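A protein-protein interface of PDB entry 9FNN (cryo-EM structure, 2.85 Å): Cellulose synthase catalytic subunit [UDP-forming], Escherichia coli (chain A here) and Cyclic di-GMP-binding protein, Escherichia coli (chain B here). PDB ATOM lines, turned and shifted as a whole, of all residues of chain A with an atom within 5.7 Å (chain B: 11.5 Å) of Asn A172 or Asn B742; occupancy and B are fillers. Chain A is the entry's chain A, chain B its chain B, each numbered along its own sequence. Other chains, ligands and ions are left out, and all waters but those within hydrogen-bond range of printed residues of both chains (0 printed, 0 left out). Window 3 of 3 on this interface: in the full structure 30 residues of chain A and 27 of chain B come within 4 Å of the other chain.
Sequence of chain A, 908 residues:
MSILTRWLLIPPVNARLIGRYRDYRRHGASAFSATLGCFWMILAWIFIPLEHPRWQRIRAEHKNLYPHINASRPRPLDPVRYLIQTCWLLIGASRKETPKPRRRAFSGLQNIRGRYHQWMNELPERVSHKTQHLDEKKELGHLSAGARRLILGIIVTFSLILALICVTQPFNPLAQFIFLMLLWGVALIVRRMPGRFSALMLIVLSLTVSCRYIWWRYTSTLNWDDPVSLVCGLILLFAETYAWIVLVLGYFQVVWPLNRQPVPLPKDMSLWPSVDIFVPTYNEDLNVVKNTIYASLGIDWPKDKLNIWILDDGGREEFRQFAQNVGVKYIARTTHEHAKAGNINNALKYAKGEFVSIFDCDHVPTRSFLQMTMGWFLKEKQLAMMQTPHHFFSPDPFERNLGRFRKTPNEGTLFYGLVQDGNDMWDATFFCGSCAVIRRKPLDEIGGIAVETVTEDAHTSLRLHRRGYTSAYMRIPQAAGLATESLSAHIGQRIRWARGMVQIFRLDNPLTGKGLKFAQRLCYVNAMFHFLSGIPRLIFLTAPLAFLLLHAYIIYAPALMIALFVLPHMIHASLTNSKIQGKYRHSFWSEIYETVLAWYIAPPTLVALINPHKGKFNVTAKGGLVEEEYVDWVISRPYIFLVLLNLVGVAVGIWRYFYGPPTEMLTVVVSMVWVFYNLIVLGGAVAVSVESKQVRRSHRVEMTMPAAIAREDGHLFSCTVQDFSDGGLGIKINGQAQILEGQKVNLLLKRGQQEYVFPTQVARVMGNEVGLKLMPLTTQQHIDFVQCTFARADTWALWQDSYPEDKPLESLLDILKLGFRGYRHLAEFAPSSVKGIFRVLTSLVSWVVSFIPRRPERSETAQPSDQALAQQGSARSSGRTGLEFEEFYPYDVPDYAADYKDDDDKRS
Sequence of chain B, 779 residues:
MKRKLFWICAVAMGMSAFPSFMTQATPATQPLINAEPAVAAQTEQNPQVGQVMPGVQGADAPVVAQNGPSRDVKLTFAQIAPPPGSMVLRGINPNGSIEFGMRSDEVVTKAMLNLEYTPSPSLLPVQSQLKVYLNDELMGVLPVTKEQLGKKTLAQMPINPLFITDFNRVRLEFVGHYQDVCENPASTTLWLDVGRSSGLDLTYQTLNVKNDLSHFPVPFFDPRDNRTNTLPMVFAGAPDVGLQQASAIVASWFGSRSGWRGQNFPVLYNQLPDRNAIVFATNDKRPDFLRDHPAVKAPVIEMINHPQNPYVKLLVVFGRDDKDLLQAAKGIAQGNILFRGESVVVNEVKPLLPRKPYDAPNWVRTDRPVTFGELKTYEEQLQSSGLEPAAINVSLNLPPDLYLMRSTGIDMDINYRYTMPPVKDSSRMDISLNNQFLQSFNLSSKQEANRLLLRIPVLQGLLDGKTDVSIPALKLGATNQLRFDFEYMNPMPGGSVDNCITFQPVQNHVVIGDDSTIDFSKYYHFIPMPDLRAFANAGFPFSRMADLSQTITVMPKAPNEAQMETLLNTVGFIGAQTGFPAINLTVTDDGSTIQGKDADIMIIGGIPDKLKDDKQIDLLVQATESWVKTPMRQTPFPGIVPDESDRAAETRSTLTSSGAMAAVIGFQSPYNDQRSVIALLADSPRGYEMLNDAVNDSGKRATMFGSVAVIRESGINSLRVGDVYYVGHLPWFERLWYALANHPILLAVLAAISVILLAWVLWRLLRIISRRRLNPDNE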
ATOM      1  N   PRO A 170      -5.632 -16.367  -5.821  1.00  0.00           N
ATOM      2  CA  PRO A 170      -5.921 -14.934  -5.729  1.00  0.00           C
ATOM      3  C   PRO A 170      -7.242 -14.610  -6.404  1.00  0.00           C
ATOM      4  O   PRO A 170      -7.651 -15.263  -7.364  1.00  0.00           O
ATOM      5  CB  PRO A 170      -4.742 -14.285  -6.457  1.00  0.00           C
ATOM      6  CG  PRO A 170      -4.250 -15.345  -7.376  1.00  0.00           C
ATOM      7  CD  PRO A 170      -4.431 -16.629  -6.626  1.00  0.00           C
ATOM      8  N   PHE A 171      -7.909 -13.589  -5.882  1.00  0.00           N
ATOM      9  CA  PHE A 171      -9.224 -13.187  -6.342  1.00  0.00           C
ATOM     10  C   PHE A 171      -9.280 -11.672  -6.474  1.00  0.00           C
ATOM     11  O   PHE A 171      -8.446 -10.948  -5.928  1.00  0.00           O
ATOM     12  CB  PHE A 171     -10.318 -13.625  -5.367  1.00  0.00           C
ATOM     13  CG  PHE A 171     -10.875 -14.978  -5.634  1.00  0.00           C
ATOM     14  CD1 PHE A 171     -11.046 -15.434  -6.919  1.00  0.00           C
ATOM     15  CD2 PHE A 171     -11.258 -15.785  -4.581  1.00  0.00           C
ATOM     16  CE1 PHE A 171     -11.576 -16.662  -7.149  1.00  0.00           C
ATOM     17  CE2 PHE A 171     -11.782 -17.016  -4.806  1.00  0.00           C
ATOM     18  CZ  PHE A 171     -11.937 -17.459  -6.097  1.00  0.00           C
ATOM     19  N   ASN A 172     -10.297 -11.197  -7.235  1.00  0.00           N
ATOM     20  CA  ASN A 172     -10.859  -9.855  -7.198  1.00  0.00           C
ATOM     21  C   ASN A 172     -12.021  -9.819  -6.204  1.00  0.00           C
ATOM     22  O   ASN A 172     -12.664 -10.845  -5.962  1.00  0.00           O
ATOM     23  CB  ASN A 172     -11.346  -9.443  -8.583  1.00  0.00           C
ATOM     24  CG  ASN A 172     -12.435 -10.355  -9.116  1.00  0.00           C
ATOM     25  OD1 ASN A 172     -13.623 -10.106  -8.911  1.00  0.00           O
ATOM     26  ND2 ASN A 172     -12.034 -11.417  -9.805  1.00  0.00           N
ATOM     27  N   PRO A 173     -12.331  -8.663  -5.610  1.00  0.00           N
ATOM     28  CA  PRO A 173     -13.309  -8.657  -4.506  1.00  0.00           C
ATOM     29  C   PRO A 173     -14.656  -9.292  -4.824  1.00  0.00           C
ATOM     30  O   PRO A 173     -15.210  -9.977  -3.957  1.00  0.00           O
ATOM     31  CB  PRO A 173     -13.441  -7.165  -4.190  1.00  0.00           C
ATOM     32  CG  PRO A 173     -12.092  -6.636  -4.477  1.00  0.00           C
ATOM     33  CD  PRO A 173     -11.633  -7.371  -5.714  1.00  0.00           C
ATOM     34  N   LEU A 174     -15.198  -9.107  -6.030  1.00  0.00           N
ATOM     35  CA  LEU A 174     -16.480  -9.732  -6.352  1.00  0.00           C
ATOM     36  C   LEU A 174     -16.369 -11.253  -6.366  1.00  0.00           C
ATOM     37  O   LEU A 174     -17.254 -11.952  -5.853  1.00  0.00           O
ATOM     38  CB  LEU A 174     -16.995  -9.213  -7.697  1.00  0.00           C
ATOM     39  CG  LEU A 174     -18.441  -9.506  -8.119  1.00  0.00           C
ATOM     40  CD1 LEU A 174     -18.573 -10.842  -8.846  1.00  0.00           C
ATOM     41  CD2 LEU A 174     -19.381  -9.451  -6.919  1.00  0.00           C
ATOM     42  N   ALA A 175     -15.292 -11.783  -6.952  1.00  0.00           N
ATOM     43  CA  ALA A 175     -15.099 -13.230  -6.981  1.00  0.00           C
ATOM     44  C   ALA A 175     -14.941 -13.791  -5.575  1.00  0.00           C
ATOM     45  O   ALA A 175     -15.510 -14.842  -5.245  1.00  0.00           O
ATOM     46  CB  ALA A 175     -13.883 -13.579  -7.838  1.00  0.00           C
ATOM     47  N   GLN A 176     -14.169 -13.103  -4.732  1.00  0.00           N
ATOM     48  CA  GLN A 176     -14.031 -13.528  -3.346  1.00  0.00           C
ATOM     49  C   GLN A 176     -15.372 -13.506  -2.629  1.00  0.00           C
ATOM     50  O   GLN A 176     -15.673 -14.407  -1.843  1.00  0.00           O
ATOM     51  CB  GLN A 176     -13.022 -12.644  -2.621  1.00  0.00           C
ATOM     52  CG  GLN A 176     -12.999 -12.827  -1.115  1.00  0.00           C
ATOM     53  CD  GLN A 176     -12.294 -14.092  -0.675  1.00  0.00           C
ATOM     54  OE1 GLN A 176     -11.998 -14.971  -1.482  1.00  0.00           O
ATOM     55  NE2 GLN A 176     -12.008 -14.185   0.618  1.00  0.00           N
ATOM     56  N   PHE A 177     -16.194 -12.488  -2.884  1.00  0.00           N
ATOM     57  CA  PHE A 177     -17.496 -12.422  -2.231  1.00  0.00           C
ATOM     58  C   PHE A 177     -18.391 -13.575  -2.662  1.00  0.00           C
ATOM     59  O   PHE A 177     -19.121 -14.147  -1.842  1.00  0.00           O
ATOM     60  CB  PHE A 177     -18.169 -11.084  -2.525  1.00  0.00           C
ATOM     61  CG  PHE A 177     -19.383 -10.824  -1.688  1.00  0.00           C
ATOM     62  CD1 PHE A 177     -19.266 -10.230  -0.447  1.00  0.00           C
ATOM     63  CD2 PHE A 177     -20.641 -11.172  -2.141  1.00  0.00           C
ATOM     64  CE1 PHE A 177     -20.379  -9.988   0.327  1.00  0.00           C
ATOM     65  CE2 PHE A 177     -21.758 -10.934  -1.372  1.00  0.00           C
ATOM     66  CZ  PHE A 177     -21.627 -10.341  -0.137  1.00  0.00           C
ATOM     67  N   MET A 561     -11.091  -5.930   1.498  1.00  0.00           N
ATOM     68  CA  MET A 561     -10.423  -7.227   1.440  1.00  0.00           C
ATOM     69  C   MET A 561     -10.256  -7.829   2.830  1.00  0.00           C
ATOM     70  O   MET A 561     -10.381  -9.048   3.005  1.00  0.00           O
ATOM     71  CB  MET A 561      -9.074  -7.094   0.741  1.00  0.00           C
ATOM     72  CG  MET A 561      -9.182  -6.697  -0.716  1.00  0.00           C
ATOM     73  SD  MET A 561     -10.058  -7.912  -1.708  1.00  0.00           S
ATOM     74  CE  MET A 561      -8.885  -9.262  -1.690  1.00  0.00           C
ATOM     75  N   GLU B 734       1.337 -19.302 -11.586  1.00  0.00           N
ATOM     76  CA  GLU B 734       0.699 -18.192 -12.282  1.00  0.00           C
ATOM     77  C   GLU B 734      -0.295 -18.700 -13.318  1.00  0.00           C
ATOM     78  O   GLU B 734      -1.395 -18.153 -13.455  1.00  0.00           O
ATOM     79  CB  GLU B 734       1.752 -17.307 -12.945  1.00  0.00           C
ATOM     80  CG  GLU B 734       2.804 -16.761 -11.997  1.00  0.00           C
ATOM     81  CD  GLU B 734       3.880 -15.971 -12.717  1.00  0.00           C
ATOM     82  OE1 GLU B 734       3.771 -15.803 -13.950  1.00  0.00           O
ATOM     83  OE2 GLU B 734       4.835 -15.519 -12.051  1.00  0.00           O
ATOM     84  N   ARG B 735       0.079 -19.743 -14.063  1.00  0.00           N
ATOM     85  CA  ARG B 735      -0.823 -20.302 -15.062  1.00  0.00           C
ATOM     86  C   ARG B 735      -2.073 -20.882 -14.416  1.00  0.00           C
ATOM     87  O   ARG B 735      -3.188 -20.688 -14.918  1.00  0.00           O
ATOM     88  CB  ARG B 735      -0.099 -21.370 -15.878  1.00  0.00           C
ATOM     89  CG  ARG B 735       1.022 -20.833 -16.747  1.00  0.00           C
ATOM     90  CD  ARG B 735       1.532 -21.904 -17.693  1.00  0.00           C
ATOM     91  NE  ARG B 735       2.567 -21.401 -18.589  1.00  0.00           N
ATOM     92  CZ  ARG B 735       3.136 -22.117 -19.548  1.00  0.00           C
ATOM     93  NH1 ARG B 735       2.791 -23.374 -19.769  1.00  0.00           N
ATOM     94  NH2 ARG B 735       4.075 -21.557 -20.306  1.00  0.00           N
ATOM     95  N   LEU B 736      -1.908 -21.599 -13.304  1.00  0.00           N
ATOM     96  CA  LEU B 736      -3.061 -22.174 -12.621  1.00  0.00           C
ATOM     97  C   LEU B 736      -3.977 -21.086 -12.081  1.00  0.00           C
ATOM     98  O   LEU B 736      -5.206 -21.200 -12.167  1.00  0.00           O
ATOM     99  CB  LEU B 736      -2.598 -23.097 -11.496  1.00  0.00           C
ATOM    100  CG  LEU B 736      -3.705 -23.815 -10.723  1.00  0.00           C
ATOM    101  CD1 LEU B 736      -4.510 -24.710 -11.649  1.00  0.00           C
ATOM    102  CD2 LEU B 736      -3.119 -24.615  -9.573  1.00  0.00           C
ATOM    103  N   TRP B 737      -3.398 -20.024 -11.516  1.00  0.00           N
ATOM    104  CA  TRP B 737      -4.214 -18.923 -11.014  1.00  0.00           C
ATOM    105  C   TRP B 737      -4.958 -18.229 -12.146  1.00  0.00           C
ATOM    106  O   TRP B 737      -6.152 -17.928 -12.021  1.00  0.00           O
ATOM    107  CB  TRP B 737      -3.338 -17.931 -10.252  1.00  0.00           C
ATOM    108  CG  TRP B 737      -2.729 -18.513  -9.024  1.00  0.00           C
ATOM    109  CD1 TRP B 737      -3.076 -19.676  -8.417  1.00  0.00           C
ATOM    110  CD2 TRP B 737      -1.655 -17.963  -8.257  1.00  0.00           C
ATOM    111  NE1 TRP B 737      -2.291 -19.889  -7.315  1.00  0.00           N
ATOM    112  CE2 TRP B 737      -1.408 -18.850  -7.195  1.00  0.00           C
ATOM    113  CE3 TRP B 737      -0.876 -16.809  -8.366  1.00  0.00           C
ATOM    114  CZ2 TRP B 737      -0.418 -18.620  -6.248  1.00  0.00           C
ATOM    115  CZ3 TRP B 737       0.104 -16.581  -7.423  1.00  0.00           C
ATOM    116  CH2 TRP B 737       0.326 -17.483  -6.377  1.00  0.00           C
ATOM    117  N   TYR B 738      -4.276 -17.982 -13.266  1.00  0.00           N
ATOM    118  CA  TYR B 738      -4.922 -17.339 -14.402  1.00  0.00           C
ATOM    119  C   TYR B 738      -6.000 -18.225 -15.006  1.00  0.00           C
ATOM    120  O   TYR B 738      -6.952 -17.717 -15.609  1.00  0.00           O
ATOM    121  CB  TYR B 738      -3.884 -16.971 -15.457  1.00  0.00           C
ATOM    122  CG  TYR B 738      -4.333 -15.880 -16.400  1.00  0.00           C
ATOM    123  CD1 TYR B 738      -4.106 -14.543 -16.101  1.00  0.00           C
ATOM    124  CD2 TYR B 738      -4.982 -16.184 -17.589  1.00  0.00           C
ATOM    125  CE1 TYR B 738      -4.514 -13.539 -16.959  1.00  0.00           C
ATOM    126  CE2 TYR B 738      -5.394 -15.186 -18.454  1.00  0.00           C
ATOM    127  CZ  TYR B 738      -5.157 -13.866 -18.133  1.00  0.00           C
ATOM    128  OH  TYR B 738      -5.564 -12.870 -18.990  1.00  0.00           O
ATOM    129  N   ALA B 739      -5.869 -19.546 -14.864  1.00  0.00           N
ATOM    130  CA  ALA B 739      -6.911 -20.439 -15.352  1.00  0.00           C
ATOM    131  C   ALA B 739      -8.229 -20.193 -14.629  1.00  0.00           C
ATOM    132  O   ALA B 739      -9.294 -20.155 -15.256  1.00  0.00           O
ATOM    133  CB  ALA B 739      -6.472 -21.894 -15.193  1.00  0.00           C
ATOM    134  N   LEU B 740      -8.177 -20.013 -13.312  1.00  0.00           N
ATOM    135  CA  LEU B 740      -9.362 -19.793 -12.489  1.00  0.00           C
ATOM    136  C   LEU B 740      -9.351 -18.401 -11.866  1.00  0.00           C
ATOM    137  O   LEU B 740      -9.665 -18.226 -10.687  1.00  0.00           O
ATOM    138  CB  LEU B 740      -9.479 -20.856 -11.399  1.00  0.00           C
ATOM    139  CG  LEU B 740      -9.574 -22.330 -11.797  1.00  0.00           C
ATOM    140  CD1 LEU B 740      -8.191 -22.942 -11.964  1.00  0.00           C
ATOM    141  CD2 LEU B 740     -10.383 -23.104 -10.771  1.00  0.00           C
ATOM    142  N   ALA B 741      -8.975 -17.394 -12.658  1.00  0.00           N
ATOM    143  CA  ALA B 741      -8.878 -16.035 -12.136  1.00  0.00           C
ATOM    144  C   ALA B 741     -10.238 -15.495 -11.714  1.00  0.00           C
ATOM    145  O   ALA B 741     -10.350 -14.814 -10.689  1.00  0.00           O
ATOM    146  CB  ALA B 741      -8.238 -15.118 -13.177  1.00  0.00           C
ATOM    147  N   ASN B 742     -11.281 -15.787 -12.483  1.00  0.00           N
ATOM    148  CA  ASN B 742     -12.606 -15.220 -12.258  1.00  0.00           C
ATOM    149  C   ASN B 742     -13.670 -16.306 -12.320  1.00  0.00           C
ATOM    150  O   ASN B 742     -14.694 -16.170 -12.994  1.00  0.00           O
ATOM    151  CB  ASN B 742     -12.904 -14.117 -13.268  1.00  0.00           C
ATOM    152  CG  ASN B 742     -11.944 -12.949 -13.160  1.00  0.00           C
ATOM    153  OD1 ASN B 742     -11.505 -12.591 -12.068  1.00  0.00           O
ATOM    154  ND2 ASN B 742     -11.614 -12.347 -14.296  1.00  0.00           N
ATOM    155  N   HIS B 743     -13.440 -17.412 -11.617  1.00  0.00           N
ATOM    156  CA  HIS B 743     -14.392 -18.521 -11.554  1.00  0.00           C
ATOM    157  C   HIS B 743     -14.642 -18.893 -10.099  1.00  0.00           C
ATOM    158  O   HIS B 743     -14.021 -19.821  -9.565  1.00  0.00           O
ATOM    159  CB  HIS B 743     -13.891 -19.721 -12.358  1.00  0.00           C
ATOM    160  CG  HIS B 743     -13.868 -19.485 -13.835  1.00  0.00           C
ATOM    161  ND1 HIS B 743     -12.714 -19.186 -14.524  1.00  0.00           N
ATOM    162  CD2 HIS B 743     -14.862 -19.501 -14.753  1.00  0.00           C
ATOM    163  CE1 HIS B 743     -12.995 -19.032 -15.805  1.00  0.00           C
ATOM    164  NE2 HIS B 743     -14.292 -19.217 -15.970  1.00  0.00           N
ATOM    165  N   PRO B 744     -15.547 -18.186  -9.427  1.00  0.00           N
ATOM    166  CA  PRO B 744     -15.848 -18.516  -8.029  1.00  0.00           C
ATOM    167  C   PRO B 744     -16.747 -19.734  -7.880  1.00  0.00           C
ATOM    168  O   PRO B 744     -16.599 -20.501  -6.924  1.00  0.00           O
ATOM    169  CB  PRO B 744     -16.533 -17.245  -7.516  1.00  0.00           C
ATOM    170  CG  PRO B 744     -17.150 -16.648  -8.722  1.00  0.00           C
ATOM    171  CD  PRO B 744     -16.235 -16.964  -9.870  1.00  0.00           C
ATOM    172  N   ILE B 745     -17.680 -19.926  -8.816  1.00  0.00           N
ATOM    173  CA  ILE B 745     -18.587 -21.069  -8.745  1.00  0.00           C
ATOM    174  C   ILE B 745     -17.815 -22.377  -8.883  1.00  0.00           C
ATOM    175  O   ILE B 745     -18.029 -23.330  -8.121  1.00  0.00           O
ATOM    176  CB  ILE B 745     -19.684 -20.943  -9.817  1.00  0.00           C
ATOM    177  CG1 ILE B 745     -20.773 -19.973  -9.358  1.00  0.00           C
ATOM    178  CG2 ILE B 745     -20.277 -22.307 -10.145  1.00  0.00           C
ATOM    179  CD1 ILE B 745     -21.767 -20.580  -8.398  1.00  0.00           C
ATOM    180  N   LEU B 746     -16.897 -22.439  -9.848  1.00  0.00           N
ATOM    181  CA  LEU B 746     -16.118 -23.655 -10.055  1.00  0.00           C
ATOM    182  C   LEU B 746     -15.237 -23.963  -8.851  1.00  0.00           C
ATOM    183  O   LEU B 746     -15.108 -25.125  -8.447  1.00  0.00           O
ATOM    184  CB  LEU B 746     -15.268 -23.523 -11.317  1.00  0.00           C
ATOM    185  CG  LEU B 746     -14.439 -24.749 -11.690  1.00  0.00           C
ATOM    186  CD1 LEU B 746     -15.345 -25.946 -11.913  1.00  0.00           C
ATOM    187  CD2 LEU B 746     -13.599 -24.471 -12.925  1.00  0.00           C
ATOM    188  N   LEU B 747     -14.613 -22.933  -8.273  1.00  0.00           N
ATOM    189  CA  LEU B 747     -13.763 -23.152  -7.108  1.00  0.00           C
ATOM    190  C   LEU B 747     -14.585 -23.571  -5.899  1.00  0.00           C
ATOM    191  O   LEU B 747     -14.130 -24.384  -5.088  1.00  0.00           O
ATOM    192  CB  LEU B 747     -12.946 -21.902  -6.793  1.00  0.00           C
ATOM    193  CG  LEU B 747     -11.663 -22.230  -6.023  1.00  0.00           C
ATOM    194  CD1 LEU B 747     -10.625 -22.837  -6.951  1.00  0.00           C
ATOM    195  CD2 LEU B 747     -11.090 -21.021  -5.305  1.00  0.00           C
ATOM    196  N   ALA B 748     -15.792 -23.024  -5.755  1.00  0.00           N
ATOM    197  CA  ALA B 748     -16.679 -23.479  -4.692  1.00  0.00           C
ATOM    198  C   ALA B 748     -17.039 -24.946  -4.872  1.00  0.00           C
ATOM    199  O   ALA B 748     -17.069 -25.712  -3.901  1.00  0.00           O
ATOM    200  CB  ALA B 748     -17.939 -22.618  -4.657  1.00  0.00           C
ATOM    201  N   LEU B 750     -15.225 -27.235  -6.444  1.00  0.00           N
ATOM    202  CA  LEU B 750     -14.029 -28.020  -6.147  1.00  0.00           C
ATOM    203  C   LEU B 750     -13.787 -28.117  -4.645  1.00  0.00           C
ATOM    204  O   LEU B 750     -13.436 -29.187  -4.130  1.00  0.00           O
ATOM    205  CB  LEU B 750     -12.811 -27.413  -6.840  1.00  0.00           C
ATOM    206  CG  LEU B 750     -12.792 -27.431  -8.366  1.00  0.00           C
ATOM    207  CD1 LEU B 750     -11.526 -26.772  -8.880  1.00  0.00           C
ATOM    208  CD2 LEU B 750     -12.909 -28.851  -8.884  1.00  0.00           C
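OD1 of Asn A172 sits close to N of Leu A174 (3.4 Å).
OD1 of Asn A172 is in hydrogen-bond range of N of Ala A175, at 3.1 Å.
Printed residues of chain A that touch a printed residue of chain B: Pro A170, Phe A171, Asn A172 and Ala A175.
Hydrophobic or aromatic side chains of chain B that line the printed part of chain A: Trp B737, Pro B744 and Leu B747.
Along chain B the printed residues that touch a printed residue of chain A span positions 737 to 747.
Among the printed residues, no Asp or Glu carboxylate lies within 4 Å of a Lys or Arg side-chain nitrogen of the other chain.
OD1 of Asn B742 is in hydrogen-bond range of ND2 of Asn A172, 2.6 Å away.
Of the printed residues of chain B, Phe A171 touches Ala B741 (3.9 Å) and Leu B747 (3.7 Å).
Asn A172 touches two residues of chain B.
No residue of chain B comes within 4 Å of Pro A173.
No residue of chain B comes within 4 Å of Leu A174.
No residue of chain B comes within 4 Å of Gln A176.
Of the printed residues of chain A, Ala B741 touches Phe A171 and Asn A172.
Of the printed residues of chain A, Asn B742 touches Asn A172.
His B743 touches none of the printed residues of chain A.
Of the printed residues of chain A, Leu B747 touches Phe A171 (3.7 Å).
The nearest residue of chain B that does not touch Asn A172 is His B743 (6.4 Å).
The nearest residue of chain A that does not touch Asn B742 is Ala A175 (4.9 Å).
The nearest printed residue of chain B that does not touch Pro A170 is Ala B741 (4.3 Å).
Trp B737 touches Pro A170.
Phe A171 touches Ala B741 (CD1 to O, 3.9 Å).
CZ of Phe A171 touches CD2 of Leu B747, at 3.7 Å.
Ala B741 touches Asn A172.
Ala A175 touches Pro B744.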
